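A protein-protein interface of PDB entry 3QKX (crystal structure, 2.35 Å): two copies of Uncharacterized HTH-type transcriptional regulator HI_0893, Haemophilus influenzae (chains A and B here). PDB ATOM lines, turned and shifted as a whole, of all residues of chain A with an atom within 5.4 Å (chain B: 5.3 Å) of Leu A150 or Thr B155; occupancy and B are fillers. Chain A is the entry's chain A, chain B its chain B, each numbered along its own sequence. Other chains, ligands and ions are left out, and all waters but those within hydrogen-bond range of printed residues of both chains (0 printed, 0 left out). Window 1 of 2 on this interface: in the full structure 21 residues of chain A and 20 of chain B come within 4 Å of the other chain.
The side-chain carboxylate (OD2) of Asp A146 lies within salt-bridge range of the side-chain amino group (NZ) of Lys B164. The backbone carbonyl oxygen (O) of Leu A150 sits at hydrogen-bond distance from the side-chain amide nitrogen (ND2) of Asn B158.
The backbone carbonyl oxygen of Phe A149 sits at hydrogen-bond distance from the backbone NH of Lys A154 (3.0 Å). OG1 of Thr B155 is in hydrogen-bond range of NE1 of Trp B89, 3.0 Å away. The side-chain hydroxyl of Thr B155 sits at hydrogen-bond distance from the backbone carbonyl oxygen of Ser B152. The backbone carbonyl oxygen (O) of Lys B154 lies close to the side-chain amide oxygen (OD1) of Asn B158 (3.4 Å). The side-chain hydroxyl (OG) of Ser B182 is in hydrogen-bond range of the backbone carbonyl oxygen (O) of Val B178, at 3.1 Å.
Among the printed residues, pairs that only touch across the chains: Lys A154 with Asn B158 (3.4 Å), Leu A151 with Thr B155 (3.8 Å), Leu A150 with Leu B159 (3.9 Å), Ile A147 with Leu B159 (3.9 Å), Ile A147 with Val B178 (3.9 Å) and Leu A150 with Thr B155 (3.996 Å).
Of the printed residues of chain B, Ile A147 touches Leu B159 and Val B178. Printed residues of chain B within 4 Å of Leu A151: Thr B155. Printed residues of chain A within 4 Å of Thr B155: Leu A150 and Leu A151. Printed residues of chain A within 4 Å of Asn B158: Leu A150 (3.3 Å) and Lys A154 (3.4 Å). Of the printed residues of chain A, Leu B159 touches Ile A147 and Leu A150. Of the printed residues of chain A, Lys B164 touches Asp A146.
Printed residues of chain B that touch a printed residue of chain A: Thr B155, Asn B158, Leu B159, Lys B164 and Val B178. Of the 9 printed residues of chain A, 5 touch a printed residue of chain B. Hydrophobic or aromatic side chains of chain A that line the printed part of chain B: Ile A147, Leu A150 and Leu A151. Among the printed residues, 8 pairs touch across the chains.
5 positions are printed for both chains.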
ATOM      1  N   GLU A 145     -34.767  14.340 -27.442  1.00  0.00           N
ATOM      2  CA  GLU A 145     -33.528  15.000 -26.966  1.00  0.00           C
ATOM      3  C   GLU A 145     -33.199  14.633 -25.526  1.00  0.00           C
ATOM      4  O   GLU A 145     -32.031  14.501 -25.194  1.00  0.00           O
ATOM      5  CB  GLU A 145     -33.613  16.523 -27.109  1.00  0.00           C
ATOM      6  CG  GLU A 145     -33.725  17.013 -28.572  1.00  0.00           C
ATOM      7  CD  GLU A 145     -35.168  17.157 -29.085  1.00  0.00           C
ATOM      8  OE1 GLU A 145     -36.093  16.575 -28.475  1.00  0.00           O
ATOM      9  OE2 GLU A 145     -35.367  17.856 -30.112  1.00  0.00           O
ATOM     10  N   ASP A 146     -34.212  14.442 -24.678  1.00  0.00           N
ATOM     11  CA  ASP A 146     -33.937  14.071 -23.277  1.00  0.00           C
ATOM     12  C   ASP A 146     -33.383  12.661 -23.142  1.00  0.00           C
ATOM     13  O   ASP A 146     -32.452  12.458 -22.393  1.00  0.00           O
ATOM     14  CB  ASP A 146     -35.122  14.313 -22.310  1.00  0.00           C
ATOM     15  CG  ASP A 146     -36.412  13.673 -22.758  1.00  0.00           C
ATOM     16  OD1 ASP A 146     -36.377  12.732 -23.574  1.00  0.00           O
ATOM     17  OD2 ASP A 146     -37.484  14.123 -22.284  1.00  0.00           O
ATOM     18  N   ILE A 147     -33.917  11.714 -23.919  1.00  0.00           N
ATOM     19  CA  ILE A 147     -33.401  10.349 -23.938  1.00  0.00           C
ATOM     20  C   ILE A 147     -31.954  10.352 -24.388  1.00  0.00           C
ATOM     21  O   ILE A 147     -31.089   9.753 -23.739  1.00  0.00           O
ATOM     22  CB  ILE A 147     -34.229   9.416 -24.849  1.00  0.00           C
ATOM     23  CG1 ILE A 147     -35.569   9.091 -24.202  1.00  0.00           C
ATOM     24  CG2 ILE A 147     -33.512   8.148 -25.086  1.00  0.00           C
ATOM     25  CD1 ILE A 147     -36.586   8.492 -25.157  1.00  0.00           C
ATOM     26  N   LEU A 148     -31.675  11.064 -25.465  1.00  0.00           N
ATOM     27  CA  LEU A 148     -30.306  11.161 -25.941  1.00  0.00           C
ATOM     28  C   LEU A 148     -29.378  11.716 -24.856  1.00  0.00           C
ATOM     29  O   LEU A 148     -28.296  11.171 -24.614  1.00  0.00           O
ATOM     30  CB  LEU A 148     -30.240  12.042 -27.189  1.00  0.00           C
ATOM     31  CG  LEU A 148     -30.888  11.488 -28.461  1.00  0.00           C
ATOM     32  CD1 LEU A 148     -30.873  12.581 -29.517  1.00  0.00           C
ATOM     33  CD2 LEU A 148     -30.154  10.243 -28.946  1.00  0.00           C
ATOM     34  N   PHE A 149     -29.812  12.776 -24.189  1.00  0.00           N
ATOM     35  CA  PHE A 149     -29.044  13.318 -23.077  1.00  0.00           C
ATOM     36  C   PHE A 149     -28.790  12.272 -21.997  1.00  0.00           C
ATOM     37  O   PHE A 149     -27.661  12.098 -21.581  1.00  0.00           O
ATOM     38  CB  PHE A 149     -29.743  14.508 -22.467  1.00  0.00           C
ATOM     39  CG  PHE A 149     -28.987  15.129 -21.312  1.00  0.00           C
ATOM     40  CD1 PHE A 149     -27.998  16.060 -21.540  1.00  0.00           C
ATOM     41  CD2 PHE A 149     -29.294  14.799 -20.000  1.00  0.00           C
ATOM     42  CE1 PHE A 149     -27.301  16.641 -20.476  1.00  0.00           C
ATOM     43  CE2 PHE A 149     -28.606  15.398 -18.932  1.00  0.00           C
ATOM     44  CZ  PHE A 149     -27.618  16.316 -19.179  1.00  0.00           C
ATOM     45  N   LEU A 150     -29.830  11.551 -21.598  1.00  0.00           N
ATOM     46  CA  LEU A 150     -29.746  10.613 -20.488  1.00  0.00           C
ATOM     47  C   LEU A 150     -28.906   9.370 -20.821  1.00  0.00           C
ATOM     48  O   LEU A 150     -28.438   8.686 -19.904  1.00  0.00           O
ATOM     49  CB  LEU A 150     -31.151  10.226 -19.983  1.00  0.00           C
ATOM     50  CG  LEU A 150     -31.940  11.381 -19.309  1.00  0.00           C
ATOM     51  CD1 LEU A 150     -33.419  10.973 -19.058  1.00  0.00           C
ATOM     52  CD2 LEU A 150     -31.306  11.966 -17.976  1.00  0.00           C
ATOM     53  N   LEU A 151     -28.705   9.106 -22.120  1.00  0.00           N
ATOM     54  CA  LEU A 151     -27.781   8.071 -22.607  1.00  0.00           C
ATOM     55  C   LEU A 151     -26.337   8.555 -22.777  1.00  0.00           C
ATOM     56  O   LEU A 151     -25.451   7.728 -22.960  1.00  0.00           O
ATOM     57  CB  LEU A 151     -28.251   7.504 -23.962  1.00  0.00           C
ATOM     58  CG  LEU A 151     -29.503   6.639 -24.016  1.00  0.00           C
ATOM     59  CD1 LEU A 151     -29.808   6.247 -25.457  1.00  0.00           C
ATOM     60  CD2 LEU A 151     -29.379   5.389 -23.156  1.00  0.00           C
ATOM     61  N   SER A 152     -26.093   9.867 -22.752  1.00  0.00           N
ATOM     62  CA  SER A 152     -24.789  10.403 -23.186  1.00  0.00           C
ATOM     63  C   SER A 152     -24.195  11.451 -22.196  1.00  0.00           C
ATOM     64  O   SER A 152     -23.463  11.080 -21.250  1.00  0.00           O
ATOM     65  CB  SER A 152     -24.899  10.957 -24.596  1.00  0.00           C
ATOM     66  OG  SER A 152     -25.858  12.002 -24.669  1.00  0.00           O
ATOM     67  N   LYS A 154     -25.347  12.847 -19.746  1.00  0.00           N
ATOM     68  CA  LYS A 154     -25.684  12.507 -18.371  1.00  0.00           C
ATOM     69  C   LYS A 154     -24.538  11.850 -17.640  1.00  0.00           C
ATOM     70  O   LYS A 154     -24.424  12.062 -16.458  1.00  0.00           O
ATOM     71  CB  LYS A 154     -26.910  11.616 -18.326  1.00  0.00           C
ATOM     72  CG  LYS A 154     -27.448  11.281 -16.946  1.00  0.00           C
ATOM     73  CD  LYS A 154     -27.768  12.495 -16.116  1.00  0.00           C
ATOM     74  CE  LYS A 154     -28.546  12.123 -14.864  1.00  0.00           C
ATOM     75  NZ  LYS A 154     -28.805  13.297 -13.977  1.00  0.00           N
ATOM     76  N   TYR B  85     -27.928  -8.894 -19.085  1.00  0.00           N
ATOM     77  CA  TYR B  85     -27.911  -7.453 -18.927  1.00  0.00           C
ATOM     78  C   TYR B  85     -29.284  -6.856 -19.154  1.00  0.00           C
ATOM     79  O   TYR B  85     -29.728  -5.983 -18.409  1.00  0.00           O
ATOM     80  CB  TYR B  85     -26.897  -6.817 -19.876  1.00  0.00           C
ATOM     81  CG  TYR B  85     -26.969  -5.300 -19.886  1.00  0.00           C
ATOM     82  CD1 TYR B  85     -26.270  -4.556 -18.974  1.00  0.00           C
ATOM     83  CD2 TYR B  85     -27.760  -4.629 -20.806  1.00  0.00           C
ATOM     84  CE1 TYR B  85     -26.350  -3.186 -18.957  1.00  0.00           C
ATOM     85  CE2 TYR B  85     -27.854  -3.253 -20.797  1.00  0.00           C
ATOM     86  CZ  TYR B  85     -27.150  -2.528 -19.868  1.00  0.00           C
ATOM     87  OH  TYR B  85     -27.228  -1.144 -19.880  1.00  0.00           O
ATOM     88  N   TRP B  89     -31.549  -4.668 -16.391  1.00  0.00           N
ATOM     89  CA  TRP B  89     -32.076  -3.376 -16.797  1.00  0.00           C
ATOM     90  C   TRP B  89     -33.569  -3.352 -16.584  1.00  0.00           C
ATOM     91  O   TRP B  89     -34.086  -2.412 -15.994  1.00  0.00           O
ATOM     92  CB  TRP B  89     -31.749  -3.087 -18.281  1.00  0.00           C
ATOM     93  CG  TRP B  89     -31.767  -1.637 -18.658  1.00  0.00           C
ATOM     94  CD1 TRP B  89     -30.697  -0.858 -18.891  1.00  0.00           C
ATOM     95  CD2 TRP B  89     -32.908  -0.818 -18.891  1.00  0.00           C
ATOM     96  NE1 TRP B  89     -31.087   0.411 -19.216  1.00  0.00           N
ATOM     97  CE2 TRP B  89     -32.449   0.454 -19.216  1.00  0.00           C
ATOM     98  CE3 TRP B  89     -34.276  -1.038 -18.853  1.00  0.00           C
ATOM     99  CZ2 TRP B  89     -33.291   1.482 -19.507  1.00  0.00           C
ATOM    100  CZ3 TRP B  89     -35.109   0.005 -19.111  1.00  0.00           C
ATOM    101  CH2 TRP B  89     -34.624   1.244 -19.436  1.00  0.00           C
ATOM    102  N   PHE B 149     -20.998   0.232 -14.925  1.00  0.00           N
ATOM    103  CA  PHE B 149     -22.362   0.362 -14.445  1.00  0.00           C
ATOM    104  C   PHE B 149     -22.956   1.698 -14.869  1.00  0.00           C
ATOM    105  O   PHE B 149     -24.097   1.768 -15.327  1.00  0.00           O
ATOM    106  CB  PHE B 149     -22.447   0.238 -12.917  1.00  0.00           C
ATOM    107  CG  PHE B 149     -23.867   0.360 -12.384  1.00  0.00           C
ATOM    108  CD1 PHE B 149     -24.391   1.577 -12.061  1.00  0.00           C
ATOM    109  CD2 PHE B 149     -24.658  -0.762 -12.240  1.00  0.00           C
ATOM    110  CE1 PHE B 149     -25.682   1.695 -11.635  1.00  0.00           C
ATOM    111  CE2 PHE B 149     -25.921  -0.671 -11.785  1.00  0.00           C
ATOM    112  CZ  PHE B 149     -26.458   0.578 -11.495  1.00  0.00           C
ATOM    113  N   LEU B 150     -22.171   2.752 -14.674  1.00  0.00           N
ATOM    114  CA  LEU B 150     -22.579   4.117 -14.954  1.00  0.00           C
ATOM    115  C   LEU B 150     -22.887   4.371 -16.436  1.00  0.00           C
ATOM    116  O   LEU B 150     -23.720   5.237 -16.767  1.00  0.00           O
ATOM    117  CB  LEU B 150     -21.469   5.072 -14.473  1.00  0.00           C
ATOM    118  CG  LEU B 150     -21.589   6.561 -14.811  1.00  0.00           C
ATOM    119  CD1 LEU B 150     -21.056   7.425 -13.678  1.00  0.00           C
ATOM    120  CD2 LEU B 150     -20.834   6.855 -16.079  1.00  0.00           C
ATOM    121  N   LEU B 151     -22.147   3.691 -17.316  1.00  0.00           N
ATOM    122  CA  LEU B 151     -22.347   3.809 -18.770  1.00  0.00           C
ATOM    123  C   LEU B 151     -23.577   2.995 -19.219  1.00  0.00           C
ATOM    124  O   LEU B 151     -24.159   3.286 -20.256  1.00  0.00           O
ATOM    125  CB  LEU B 151     -21.111   3.327 -19.518  1.00  0.00           C
ATOM    126  CG  LEU B 151     -19.904   4.260 -19.639  1.00  0.00           C
ATOM    127  CD1 LEU B 151     -18.685   3.498 -20.075  1.00  0.00           C
ATOM    128  CD2 LEU B 151     -20.202   5.364 -20.623  1.00  0.00           C
ATOM    129  N   SER B 152     -23.972   1.996 -18.423  1.00  0.00           N
ATOM    130  CA  SER B 152     -24.943   0.979 -18.864  1.00  0.00           C
ATOM    131  C   SER B 152     -26.187   0.923 -17.963  1.00  0.00           C
ATOM    132  O   SER B 152     -27.153   1.638 -18.223  1.00  0.00           O
ATOM    133  CB  SER B 152     -24.245  -0.357 -18.990  1.00  0.00           C
ATOM    134  OG  SER B 152     -23.897  -0.880 -17.727  1.00  0.00           O
ATOM    135  N   LEU B 153     -26.185   0.092 -16.922  1.00  0.00           N
ATOM    136  CA  LEU B 153     -27.411  -0.117 -16.119  1.00  0.00           C
ATOM    137  C   LEU B 153     -27.931   1.163 -15.523  1.00  0.00           C
ATOM    138  O   LEU B 153     -29.157   1.317 -15.356  1.00  0.00           O
ATOM    139  CB  LEU B 153     -27.204  -1.130 -14.970  1.00  0.00           C
ATOM    140  CG  LEU B 153     -27.291  -2.624 -15.244  1.00  0.00           C
ATOM    141  CD1 LEU B 153     -27.073  -3.451 -13.936  1.00  0.00           C
ATOM    142  CD2 LEU B 153     -28.598  -2.970 -15.953  1.00  0.00           C
ATOM    143  N   LYS B 154     -27.037   2.108 -15.240  1.00  0.00           N
ATOM    144  CA  LYS B 154     -27.437   3.401 -14.670  1.00  0.00           C
ATOM    145  C   LYS B 154     -28.453   4.117 -15.543  1.00  0.00           C
ATOM    146  O   LYS B 154     -29.240   4.916 -15.039  1.00  0.00           O
ATOM    147  CB  LYS B 154     -26.202   4.280 -14.462  1.00  0.00           C
ATOM    148  CG  LYS B 154     -26.432   5.707 -13.912  1.00  0.00           C
ATOM    149  CD  LYS B 154     -27.136   5.713 -12.560  1.00  0.00           C
ATOM    150  CE  LYS B 154     -26.856   7.006 -11.784  1.00  0.00           C
ATOM    151  NZ  LYS B 154     -27.384   6.927 -10.404  1.00  0.00           N
ATOM    152  N   THR B 155     -28.434   3.864 -16.859  1.00  0.00           N
ATOM    153  CA  THR B 155     -29.398   4.539 -17.726  1.00  0.00           C
ATOM    154  C   THR B 155     -30.861   4.247 -17.325  1.00  0.00           C
ATOM    155  O   THR B 155     -31.708   5.095 -17.515  1.00  0.00           O
ATOM    156  CB  THR B 155     -29.213   4.223 -19.235  1.00  0.00           C
ATOM    157  OG1 THR B 155     -29.337   2.819 -19.451  1.00  0.00           O
ATOM    158  CG2 THR B 155     -27.837   4.739 -19.744  1.00  0.00           C
ATOM    159  N   ALA B 156     -31.127   3.045 -16.807  1.00  0.00           N
ATOM    160  CA  ALA B 156     -32.429   2.661 -16.243  1.00  0.00           C
ATOM    161  C   ALA B 156     -32.876   3.584 -15.094  1.00  0.00           C
ATOM    162  O   ALA B 156     -34.028   4.033 -15.052  1.00  0.00           O
ATOM    163  CB  ALA B 156     -32.352   1.268 -15.754  1.00  0.00           C
ATOM    164  N   ILE B 157     -31.958   3.880 -14.171  1.00  0.00           N
ATOM    165  CA  ILE B 157     -32.241   4.860 -13.121  1.00  0.00           C
ATOM    166  C   ILE B 157     -32.365   6.231 -13.747  1.00  0.00           C
ATOM    167  O   ILE B 157     -33.271   6.967 -13.406  1.00  0.00           O
ATOM    168  CB  ILE B 157     -31.171   4.864 -12.012  1.00  0.00           C
ATOM    169  CG1 ILE B 157     -31.162   3.530 -11.274  1.00  0.00           C
ATOM    170  CG2 ILE B 157     -31.398   6.015 -11.002  1.00  0.00           C
ATOM    171  CD1 ILE B 157     -29.732   3.069 -10.916  1.00  0.00           C
ATOM    172  N   ASN B 158     -31.504   6.560 -14.696  1.00  0.00           N
ATOM    173  CA  ASN B 158     -31.549   7.887 -15.289  1.00  0.00           C
ATOM    174  C   ASN B 158     -32.909   8.146 -15.921  1.00  0.00           C
ATOM    175  O   ASN B 158     -33.471   9.227 -15.753  1.00  0.00           O
ATOM    176  CB  ASN B 158     -30.462   8.089 -16.383  1.00  0.00           C
ATOM    177  CG  ASN B 158     -29.022   8.111 -15.830  1.00  0.00           C
ATOM    178  OD1 ASN B 158     -28.807   8.272 -14.625  1.00  0.00           O
ATOM    179  ND2 ASN B 158     -28.023   7.963 -16.738  1.00  0.00           N
ATOM    180  N   LEU B 159     -33.427   7.144 -16.645  1.00  0.00           N
ATOM    181  CA  LEU B 159     -34.637   7.293 -17.425  1.00  0.00           C
ATOM    182  C   LEU B 159     -35.916   7.106 -16.597  1.00  0.00           C
ATOM    183  O   LEU B 159     -36.966   7.532 -17.020  1.00  0.00           O
ATOM    184  CB  LEU B 159     -34.636   6.306 -18.602  1.00  0.00           C
ATOM    185  CG  LEU B 159     -33.753   6.723 -19.775  1.00  0.00           C
ATOM    186  CD1 LEU B 159     -33.173   5.495 -20.545  1.00  0.00           C
ATOM    187  CD2 LEU B 159     -34.551   7.656 -20.717  1.00  0.00           C
ATOM    188  N   ALA B 160     -35.831   6.449 -15.446  1.00  0.00           N
ATOM    189  CA  ALA B 160     -37.019   6.119 -14.658  1.00  0.00           C
ATOM    190  C   ALA B 160     -37.825   7.385 -14.219  1.00  0.00           C
ATOM    191  O   ALA B 160     -37.340   8.255 -13.454  1.00  0.00           O
ATOM    192  CB  ALA B 160     -36.636   5.273 -13.479  1.00  0.00           C
ATOM    193  N   LYS B 164     -42.041   8.300 -18.704  1.00  0.00           N
ATOM    194  CA  LYS B 164     -41.261   7.362 -19.507  1.00  0.00           C
ATOM    195  C   LYS B 164     -41.659   5.891 -19.303  1.00  0.00           C
ATOM    196  O   LYS B 164     -41.442   5.078 -20.222  1.00  0.00           O
ATOM    197  CB  LYS B 164     -39.745   7.625 -19.381  1.00  0.00           C
ATOM    198  CG  LYS B 164     -39.347   8.642 -20.438  1.00  0.00           C
ATOM    199  CD  LYS B 164     -38.039   9.361 -20.205  1.00  0.00           C
ATOM    200  CE  LYS B 164     -37.872  10.543 -21.221  1.00  0.00           C
ATOM    201  NZ  LYS B 164     -39.038  11.527 -21.265  1.00  0.00           N
ATOM    202  N   VAL B 178     -32.935   1.678 -26.027  1.00  0.00           N
ATOM    203  CA  VAL B 178     -32.191   2.179 -24.894  1.00  0.00           C
ATOM    204  C   VAL B 178     -31.373   1.093 -24.179  1.00  0.00           C
ATOM    205  O   VAL B 178     -30.249   1.350 -23.750  1.00  0.00           O
ATOM    206  CB  VAL B 178     -33.140   2.873 -23.908  1.00  0.00           C
ATOM    207  CG1 VAL B 178     -32.569   2.866 -22.532  1.00  0.00           C
ATOM    208  CG2 VAL B 178     -33.429   4.286 -24.401  1.00  0.00           C
ATOM    209  N   SER B 182     -27.323   1.233 -24.344  1.00  0.00           N
ATOM    210  CA  SER B 182     -26.602   1.327 -23.094  1.00  0.00           C
ATOM    211  C   SER B 182     -25.616   0.161 -22.954  1.00  0.00           C
ATOM    212  O   SER B 182     -24.528   0.316 -22.391  1.00  0.00           O
ATOM    213  CB  SER B 182     -27.590   1.387 -21.913  1.00  0.00           C
ATOM    214  OG  SER B 182     -28.255   0.167 -21.736  1.00  0.00           O
